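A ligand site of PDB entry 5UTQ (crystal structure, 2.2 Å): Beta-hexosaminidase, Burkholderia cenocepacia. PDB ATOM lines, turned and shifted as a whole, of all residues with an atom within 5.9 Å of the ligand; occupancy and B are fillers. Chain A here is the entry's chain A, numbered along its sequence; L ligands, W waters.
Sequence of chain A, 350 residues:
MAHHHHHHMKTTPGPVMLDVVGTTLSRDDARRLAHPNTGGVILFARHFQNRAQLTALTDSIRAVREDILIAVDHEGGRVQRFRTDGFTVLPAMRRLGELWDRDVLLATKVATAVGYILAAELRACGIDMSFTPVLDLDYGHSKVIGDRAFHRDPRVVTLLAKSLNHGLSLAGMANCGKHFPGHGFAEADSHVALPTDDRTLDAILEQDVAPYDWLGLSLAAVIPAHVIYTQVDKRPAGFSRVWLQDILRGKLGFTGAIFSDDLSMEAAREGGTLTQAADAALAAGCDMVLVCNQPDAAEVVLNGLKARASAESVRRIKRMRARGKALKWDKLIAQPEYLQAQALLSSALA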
ATOM      1  N   ILE A  42     -17.071 -21.248  -9.337  1.00  0.00           N
ATOM      2  CA  ILE A  42     -18.044 -20.342  -9.948  1.00  0.00           C
ATOM      3  C   ILE A  42     -17.772 -18.937  -9.404  1.00  0.00           C
ATOM      4  O   ILE A  42     -17.574 -18.759  -8.203  1.00  0.00           O
ATOM      5  CB  ILE A  42     -19.490 -20.779  -9.660  1.00  0.00           C
ATOM      6  CG1 ILE A  42     -20.471 -19.760 -10.264  1.00  0.00           C
ATOM      7  CG2 ILE A  42     -19.722 -20.949  -8.163  1.00  0.00           C
ATOM      8  CD1 ILE A  42     -21.927 -20.198 -10.243  1.00  0.00           C
ATOM      9  N   PHE A  44     -18.652 -14.663  -9.128  1.00  0.00           N
ATOM     10  CA  PHE A  44     -19.757 -13.727  -8.976  1.00  0.00           C
ATOM     11  C   PHE A  44     -19.202 -12.308  -9.030  1.00  0.00           C
ATOM     12  O   PHE A  44     -17.988 -12.103  -9.140  1.00  0.00           O
ATOM     13  CB  PHE A  44     -20.537 -13.973  -7.680  1.00  0.00           C
ATOM     14  CG  PHE A  44     -21.284 -15.272  -7.658  1.00  0.00           C
ATOM     15  CD1 PHE A  44     -22.548 -15.371  -8.214  1.00  0.00           C
ATOM     16  CD2 PHE A  44     -20.728 -16.400  -7.087  1.00  0.00           C
ATOM     17  CE1 PHE A  44     -23.239 -16.563  -8.199  1.00  0.00           C
ATOM     18  CE2 PHE A  44     -21.415 -17.604  -7.066  1.00  0.00           C
ATOM     19  CZ  PHE A  44     -22.672 -17.684  -7.617  1.00  0.00           C
ATOM     20  N   ASP A  73     -22.184 -17.185 -14.156  1.00  0.00           N
ATOM     21  CA  ASP A  73     -23.536 -16.982 -14.670  1.00  0.00           C
ATOM     22  C   ASP A  73     -23.513 -15.766 -15.591  1.00  0.00           C
ATOM     23  O   ASP A  73     -23.778 -14.640 -15.174  1.00  0.00           O
ATOM     24  CB  ASP A  73     -24.533 -16.788 -13.532  1.00  0.00           C
ATOM     25  CG  ASP A  73     -24.676 -18.029 -12.665  1.00  0.00           C
ATOM     26  OD1 ASP A  73     -24.716 -19.147 -13.221  1.00  0.00           O
ATOM     27  OD2 ASP A  73     -24.760 -17.875 -11.428  1.00  0.00           O
ATOM     28  N   GLU A  75     -25.527 -14.840 -18.526  1.00  0.00           N
ATOM     29  CA  GLU A  75     -26.684 -15.001 -19.407  1.00  0.00           C
ATOM     30  C   GLU A  75     -26.962 -13.755 -20.219  1.00  0.00           C
ATOM     31  O   GLU A  75     -27.272 -13.862 -21.412  1.00  0.00           O
ATOM     32  CB  GLU A  75     -27.932 -15.343 -18.583  1.00  0.00           C
ATOM     33  CG  GLU A  75     -27.785 -16.531 -17.662  1.00  0.00           C
ATOM     34  CD  GLU A  75     -29.001 -16.735 -16.786  1.00  0.00           C
ATOM     35  OE1 GLU A  75     -30.094 -16.275 -17.170  1.00  0.00           O
ATOM     36  OE2 GLU A  75     -28.854 -17.359 -15.706  1.00  0.00           O
ATOM     37  N   ARG A  81     -22.492 -11.202 -14.315  1.00  0.00           N
ATOM     38  CA  ARG A  81     -21.657 -10.762 -13.198  1.00  0.00           C
ATOM     39  C   ARG A  81     -20.707  -9.650 -13.624  1.00  0.00           C
ATOM     40  O   ARG A  81     -20.508  -8.680 -12.889  1.00  0.00           O
ATOM     41  CB  ARG A  81     -20.868 -11.939 -12.636  1.00  0.00           C
ATOM     42  CG  ARG A  81     -21.696 -13.176 -12.371  1.00  0.00           C
ATOM     43  CD  ARG A  81     -22.891 -12.890 -11.489  1.00  0.00           C
ATOM     44  NE  ARG A  81     -23.739 -14.061 -11.346  1.00  0.00           N
ATOM     45  CZ  ARG A  81     -25.004 -14.033 -10.954  1.00  0.00           C
ATOM     46  NH1 ARG A  81     -25.603 -12.884 -10.678  1.00  0.00           N
ATOM     47  NH2 ARG A  81     -25.685 -15.166 -10.871  1.00  0.00           N
ATOM     48  N   PHE A 131     -22.874 -20.478 -17.407  1.00  0.00           N
ATOM     49  CA  PHE A 131     -24.085 -21.252 -17.176  1.00  0.00           C
ATOM     50  C   PHE A 131     -25.217 -20.611 -17.987  1.00  0.00           C
ATOM     51  O   PHE A 131     -26.081 -19.898 -17.470  1.00  0.00           O
ATOM     52  CB  PHE A 131     -24.402 -21.337 -15.691  1.00  0.00           C
ATOM     53  CG  PHE A 131     -23.473 -22.238 -14.927  1.00  0.00           C
ATOM     54  CD1 PHE A 131     -23.335 -23.573 -15.292  1.00  0.00           C
ATOM     55  CD2 PHE A 131     -22.737 -21.774 -13.857  1.00  0.00           C
ATOM     56  CE1 PHE A 131     -22.475 -24.414 -14.603  1.00  0.00           C
ATOM     57  CE2 PHE A 131     -21.883 -22.600 -13.165  1.00  0.00           C
ATOM     58  CZ  PHE A 131     -21.752 -23.930 -13.534  1.00  0.00           C
ATOM     59  N   VAL A 144     -38.793 -15.387 -11.306  1.00  0.00           N
ATOM     60  CA  VAL A 144     -37.356 -15.606 -11.175  1.00  0.00           C
ATOM     61  C   VAL A 144     -36.720 -15.817 -12.545  1.00  0.00           C
ATOM     62  O   VAL A 144     -35.563 -15.437 -12.764  1.00  0.00           O
ATOM     63  CB  VAL A 144     -37.076 -16.796 -10.230  1.00  0.00           C
ATOM     64  CG1 VAL A 144     -37.653 -18.089 -10.777  1.00  0.00           C
ATOM     65  CG2 VAL A 144     -35.585 -16.933  -9.973  1.00  0.00           C
ATOM     66  N   ILE A 145     -37.456 -16.405 -13.486  1.00  0.00           N
ATOM     67  CA  ILE A 145     -36.965 -16.538 -14.848  1.00  0.00           C
ATOM     68  C   ILE A 145     -37.202 -15.247 -15.623  1.00  0.00           C
ATOM     69  O   ILE A 145     -36.251 -14.581 -16.057  1.00  0.00           O
ATOM     70  CB  ILE A 145     -37.618 -17.739 -15.552  1.00  0.00           C
ATOM     71  CG1 ILE A 145     -37.380 -19.023 -14.746  1.00  0.00           C
ATOM     72  CG2 ILE A 145     -37.085 -17.889 -16.973  1.00  0.00           C
ATOM     73  CD1 ILE A 145     -35.916 -19.357 -14.483  1.00  0.00           C
ATOM     74  N   ARG A 148     -35.236 -13.701 -18.704  1.00  0.00           N
ATOM     75  CA  ARG A 148     -34.118 -14.603 -18.978  1.00  0.00           C
ATOM     76  C   ARG A 148     -34.478 -15.678 -20.001  1.00  0.00           C
ATOM     77  O   ARG A 148     -33.576 -16.351 -20.503  1.00  0.00           O
ATOM     78  CB  ARG A 148     -33.655 -15.269 -17.687  1.00  0.00           C
ATOM     79  CG  ARG A 148     -33.176 -14.304 -16.621  1.00  0.00           C
ATOM     80  CD  ARG A 148     -33.127 -14.965 -15.263  1.00  0.00           C
ATOM     81  NE  ARG A 148     -32.164 -16.060 -15.199  1.00  0.00           N
ATOM     82  CZ  ARG A 148     -32.090 -16.950 -14.218  1.00  0.00           C
ATOM     83  NH1 ARG A 148     -32.939 -16.887 -13.199  1.00  0.00           N
ATOM     84  NH2 ARG A 148     -31.174 -17.908 -14.245  1.00  0.00           N
ATOM     85  N   LYS A 178     -30.683 -24.837 -18.996  1.00  0.00           N
ATOM     86  CA  LYS A 178     -31.334 -24.811 -17.688  1.00  0.00           C
ATOM     87  C   LYS A 178     -32.698 -24.136 -17.775  1.00  0.00           C
ATOM     88  O   LYS A 178     -32.936 -23.346 -18.692  1.00  0.00           O
ATOM     89  CB  LYS A 178     -30.443 -24.076 -16.689  1.00  0.00           C
ATOM     90  CG  LYS A 178     -30.187 -22.614 -17.016  1.00  0.00           C
ATOM     91  CD  LYS A 178     -29.129 -22.014 -16.106  1.00  0.00           C
ATOM     92  CE  LYS A 178     -29.008 -20.512 -16.308  1.00  0.00           C
ATOM     93  NZ  LYS A 178     -27.960 -19.906 -15.447  1.00  0.00           N
ATOM     94  N   HIS A 179     -33.603 -24.406 -16.835  1.00  0.00           N
ATOM     95  CA  HIS A 179     -33.420 -25.340 -15.719  1.00  0.00           C
ATOM     96  C   HIS A 179     -34.305 -26.579 -15.936  1.00  0.00           C
ATOM     97  O   HIS A 179     -35.535 -26.500 -15.878  1.00  0.00           O
ATOM     98  CB  HIS A 179     -33.753 -24.655 -14.397  1.00  0.00           C
ATOM     99  CG  HIS A 179     -33.069 -23.337 -14.210  1.00  0.00           C
ATOM    100  ND1 HIS A 179     -33.397 -22.221 -14.949  1.00  0.00           N
ATOM    101  CD2 HIS A 179     -32.074 -22.957 -13.372  1.00  0.00           C
ATOM    102  CE1 HIS A 179     -32.632 -21.208 -14.583  1.00  0.00           C
ATOM    103  NE2 HIS A 179     -31.822 -21.629 -13.623  1.00  0.00           N
ATOM    104  N   HIS A 183     -38.377 -24.573 -15.793  1.00  0.00           N
ATOM    105  CA  HIS A 183     -38.721 -23.695 -14.685  1.00  0.00           C
ATOM    106  C   HIS A 183     -39.749 -22.641 -15.071  1.00  0.00           C
ATOM    107  O   HIS A 183     -40.171 -21.860 -14.211  1.00  0.00           O
ATOM    108  CB  HIS A 183     -37.460 -23.014 -14.155  1.00  0.00           C
ATOM    109  CG  HIS A 183     -37.526 -22.627 -12.708  1.00  0.00           C
ATOM    110  ND1 HIS A 183     -38.535 -21.839 -12.192  1.00  0.00           N
ATOM    111  CD2 HIS A 183     -36.706 -22.904 -11.671  1.00  0.00           C
ATOM    112  CE1 HIS A 183     -38.328 -21.656 -10.902  1.00  0.00           C
ATOM    113  NE2 HIS A 183     -37.234 -22.295 -10.557  1.00  0.00           N
ATOM    114  N   ILE A 223     -28.390 -27.951 -16.099  1.00  0.00           N
ATOM    115  CA  ILE A 223     -28.631 -27.704 -14.685  1.00  0.00           C
ATOM    116  C   ILE A 223     -30.102 -28.060 -14.414  1.00  0.00           C
ATOM    117  O   ILE A 223     -30.986 -27.506 -15.070  1.00  0.00           O
ATOM    118  CB  ILE A 223     -28.350 -26.253 -14.268  1.00  0.00           C
ATOM    119  CG1 ILE A 223     -26.850 -26.040 -14.075  1.00  0.00           C
ATOM    120  CG2 ILE A 223     -29.078 -25.894 -12.961  1.00  0.00           C
ATOM    121  CD1 ILE A 223     -26.442 -24.582 -13.950  1.00  0.00           C
ATOM    122  N   ASP A 261     -28.314 -27.227  -9.476  1.00  0.00           N
ATOM    123  CA  ASP A 261     -28.500 -25.818  -9.165  1.00  0.00           C
ATOM    124  C   ASP A 261     -27.998 -25.557  -7.751  1.00  0.00           C
ATOM    125  O   ASP A 261     -27.810 -26.474  -6.941  1.00  0.00           O
ATOM    126  CB  ASP A 261     -29.962 -25.420  -9.309  1.00  0.00           C
ATOM    127  CG  ASP A 261     -30.135 -23.933  -9.570  1.00  0.00           C
ATOM    128  OD1 ASP A 261     -29.156 -23.165  -9.382  1.00  0.00           O
ATOM    129  OD2 ASP A 261     -31.256 -23.517  -9.965  1.00  0.00           O
ATOM    130  N   ASP A 262     -27.782 -24.274  -7.450  1.00  0.00           N
ATOM    131  CA  ASP A 262     -27.159 -23.886  -6.190  1.00  0.00           C
ATOM    132  C   ASP A 262     -27.794 -24.606  -5.008  1.00  0.00           C
ATOM    133  O   ASP A 262     -28.983 -24.421  -4.717  1.00  0.00           O
ATOM    134  CB  ASP A 262     -27.277 -22.371  -6.015  1.00  0.00           C
ATOM    135  CG  ASP A 262     -26.531 -21.855  -4.808  1.00  0.00           C
ATOM    136  OD1 ASP A 262     -25.774 -22.642  -4.202  1.00  0.00           O
ATOM    137  OD2 ASP A 262     -26.686 -20.663  -4.478  1.00  0.00           O
ATOM    138  N   SER A 264     -27.084 -24.046  -1.974  1.00  0.00           N
ATOM    139  CA  SER A 264     -27.276 -23.089  -0.903  1.00  0.00           C
ATOM    140  C   SER A 264     -28.708 -22.564  -0.846  1.00  0.00           C
ATOM    141  O   SER A 264     -29.055 -21.876   0.116  1.00  0.00           O
ATOM    142  CB  SER A 264     -26.308 -21.911  -1.062  1.00  0.00           C
ATOM    143  OG  SER A 264     -24.960 -22.357  -1.007  1.00  0.00           O
ATOM    144  N   MET A 265     -29.535 -22.870  -1.838  1.00  0.00           N
ATOM    145  CA  MET A 265     -30.947 -22.549  -1.782  1.00  0.00           C
ATOM    146  C   MET A 265     -31.615 -23.456  -0.754  1.00  0.00           C
ATOM    147  O   MET A 265     -31.776 -24.659  -0.985  1.00  0.00           O
ATOM    148  CB  MET A 265     -31.584 -22.708  -3.160  1.00  0.00           C
ATOM    149  CG  MET A 265     -32.695 -21.728  -3.471  1.00  0.00           C
ATOM    150  SD  MET A 265     -34.335 -22.380  -3.124  1.00  0.00           S
ATOM    151  CE  MET A 265     -34.563 -23.444  -4.550  1.00  0.00           C
ATOM    152  N   GLU A 266     -31.993 -22.882   0.391  1.00  0.00           N
ATOM    153  CA  GLU A 266     -32.422 -23.675   1.545  1.00  0.00           C
ATOM    154  C   GLU A 266     -33.535 -24.655   1.186  1.00  0.00           C
ATOM    155  O   GLU A 266     -33.388 -25.869   1.374  1.00  0.00           O
ATOM    156  CB  GLU A 266     -32.885 -22.734   2.663  1.00  0.00           C
ATOM    157  CG  GLU A 266     -31.751 -22.121   3.476  1.00  0.00           C
ATOM    158  CD  GLU A 266     -31.347 -22.980   4.664  1.00  0.00           C
ATOM    159  OE1 GLU A 266     -32.178 -23.781   5.139  1.00  0.00           O
ATOM    160  OE2 GLU A 266     -30.190 -22.854   5.115  1.00  0.00           O
ATOM    161  N   LEU A 290     -23.242 -27.587  -6.995  1.00  0.00           N
ATOM    162  CA  LEU A 290     -22.883 -26.199  -6.788  1.00  0.00           C
ATOM    163  C   LEU A 290     -23.205 -25.780  -5.354  1.00  0.00           C
ATOM    164  O   LEU A 290     -24.330 -25.985  -4.887  1.00  0.00           O
ATOM    165  CB  LEU A 290     -23.606 -25.289  -7.780  1.00  0.00           C
ATOM    166  CG  LEU A 290     -22.913 -25.075  -9.129  1.00  0.00           C
ATOM    167  CD1 LEU A 290     -22.730 -26.397  -9.866  1.00  0.00           C
ATOM    168  CD2 LEU A 290     -23.693 -24.070  -9.975  1.00  0.00           C
ATOM    169  N   CYS A 292     -22.719 -22.240  -3.490  1.00  0.00           N
ATOM    170  CA  CYS A 292     -22.319 -20.860  -3.746  1.00  0.00           C
ATOM    171  C   CYS A 292     -22.494 -20.005  -2.507  1.00  0.00           C
ATOM    172  O   CYS A 292     -23.456 -20.187  -1.740  1.00  0.00           O
ATOM    173  CB  CYS A 292     -23.141 -20.276  -4.898  1.00  0.00           C
ATOM    174  SG  CYS A 292     -23.243 -21.344  -6.367  1.00  0.00           S
HETATM  175  C1  LIG L   1     -33.544 -20.795 -10.858  1.00  0.00           C
HETATM  176  C2  LIG L   1     -32.254 -20.038 -10.962  1.00  0.00           C
HETATM  177  O1  LIG L   1     -32.242 -18.878 -11.319  1.00  0.00           O
HETATM  178  N1  LIG L   1     -31.148 -20.733 -10.624  1.00  0.00           N
HETATM  179  C3  LIG L   1     -29.812 -20.144 -10.670  1.00  0.00           C
HETATM  180  C4  LIG L   1     -28.925 -20.730 -11.777  1.00  0.00           C
HETATM  181  O2  LIG L   1     -29.357 -20.259 -13.059  1.00  0.00           O
HETATM  182  C5  LIG L   1     -27.459 -20.395 -11.564  1.00  0.00           C
HETATM  183  O3  LIG L   1     -26.694 -20.860 -12.674  1.00  0.00           O
HETATM  184  C6  LIG L   1     -26.959 -21.036 -10.273  1.00  0.00           C
HETATM  185  C7  LIG L   1     -25.501 -20.705  -9.994  1.00  0.00           C
HETATM  186  O4  LIG L   1     -25.399 -19.354  -9.505  1.00  0.00           O
HETATM  187  O5  LIG L   1     -27.733 -20.590  -9.113  1.00  0.00           O
HETATM  188  C8  LIG L   1     -29.114 -20.163  -9.325  1.00  0.00           C
HETATM  189  N2  LIG L   1     -29.742 -19.790  -8.297  1.00  0.00           N
HETATM  190  O6  LIG L   1     -29.176 -19.760  -6.984  1.00  0.00           O
HETATM  191  C9  LIG L   1     -29.956 -19.304  -5.851  1.00  0.00           C
HETATM  192  O7  LIG L   1     -31.108 -18.958  -6.071  1.00  0.00           O
HETATM  193  N3  LIG L   1     -29.354 -19.314  -4.657  1.00  0.00           N
HETATM  194  C10 LIG L   1     -29.893 -18.932  -3.421  1.00  0.00           C
HETATM  195  C11 LIG L   1     -29.068 -19.134  -2.312  1.00  0.00           C
HETATM  196  C12 LIG L   1     -29.477 -18.804  -1.021  1.00  0.00           C
HETATM  197  C13 LIG L   1     -30.735 -18.253  -0.818  1.00  0.00           C
HETATM  198  C14 LIG L   1     -31.584 -18.032  -1.907  1.00  0.00           C
HETATM  199  C15 LIG L   1     -31.166 -18.366  -3.195  1.00  0.00           C
HETATM  200  O   HOH W   1     -32.455 -17.977  -8.354  1.00  0.00           O
HETATM  201  O   HOH W   2     -25.960 -18.689  -6.846  1.00  0.00           O
HETATM  202  O   HOH W   3     -33.825 -24.040  -9.923  1.00  0.00           O
HETATM  203  O   HOH W   4     -25.991 -18.758  -2.906  1.00  0.00           O
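The side-chain carboxylate (OD2) of Asp 73 lies within hydrogen-bond range of an oxygen (O4) of the ligand, at 2.5 Å. The side-chain amino group (NZ) of Lys 178 is in hydrogen-bond range of an oxygen (O2) of the ligand (2.8 Å). The guanidinium group (NH1) of Arg 148 sits at hydrogen-bond distance from an oxygen (O1) of the ligand, at 2.8 Å. The side-chain carboxylate of Asp 261 sits at hydrogen-bond distance from a nitrogen (N1) of the ligand (2.9 Å). An oxygen (O2) of the ligand lies within hydrogen-bond range of a ring nitrogen (NE2) of His 179 (2.9 Å). The side-chain carboxylate of Asp 262 sits at hydrogen-bond distance from a nitrogen (N3) of the ligand (3.0 Å).
The side-chain carboxylate (OD2) of Asp 73 is in salt-bridge range of the guanidinium group (NH2) of Arg 81 (2.9 Å). NZ of Lys 178 lies within hydrogen-bond range of O of Phe 131. NZ of Lys 178 is in salt-bridge range of OE2 of Glu 75 (2.7 Å). NH2 of Arg 148 lies within salt-bridge range of OE2 of Glu 75 (2.8 Å). The backbone carbonyl oxygen (O) of Val 144 is in hydrogen-bond range of the guanidinium group (NH1) of Arg 148, 3.0 Å away. N of Ser 264 lies within hydrogen-bond range of OD1 of Asp 262, 2.9 Å away. The side-chain carboxylate of Asp 262 sits at hydrogen-bond distance from the backbone NH of Cys 292, 3.2 Å away. The side-chain hydroxyl (OG) of Ser 264 sits at hydrogen-bond distance from the backbone carbonyl oxygen (O) of Cys 292 (2.7 Å).
Residues that only touch the ligand: Ile 42, Phe 44, Glu 75, Phe 131, His 183, Ile 223, Ser 264, Met 265 and Leu 290.
Water W2 bridges O4 of the ligand (2.8 Å) and OD2 of Asp 262 (3.2 Å). Water W4 lies within hydrogen-bond range of the side-chain carboxylate (OD2) of Asp 262 (2.6 Å) and the backbone carbonyl oxygen (O) of Cys 292 (3.1 Å).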
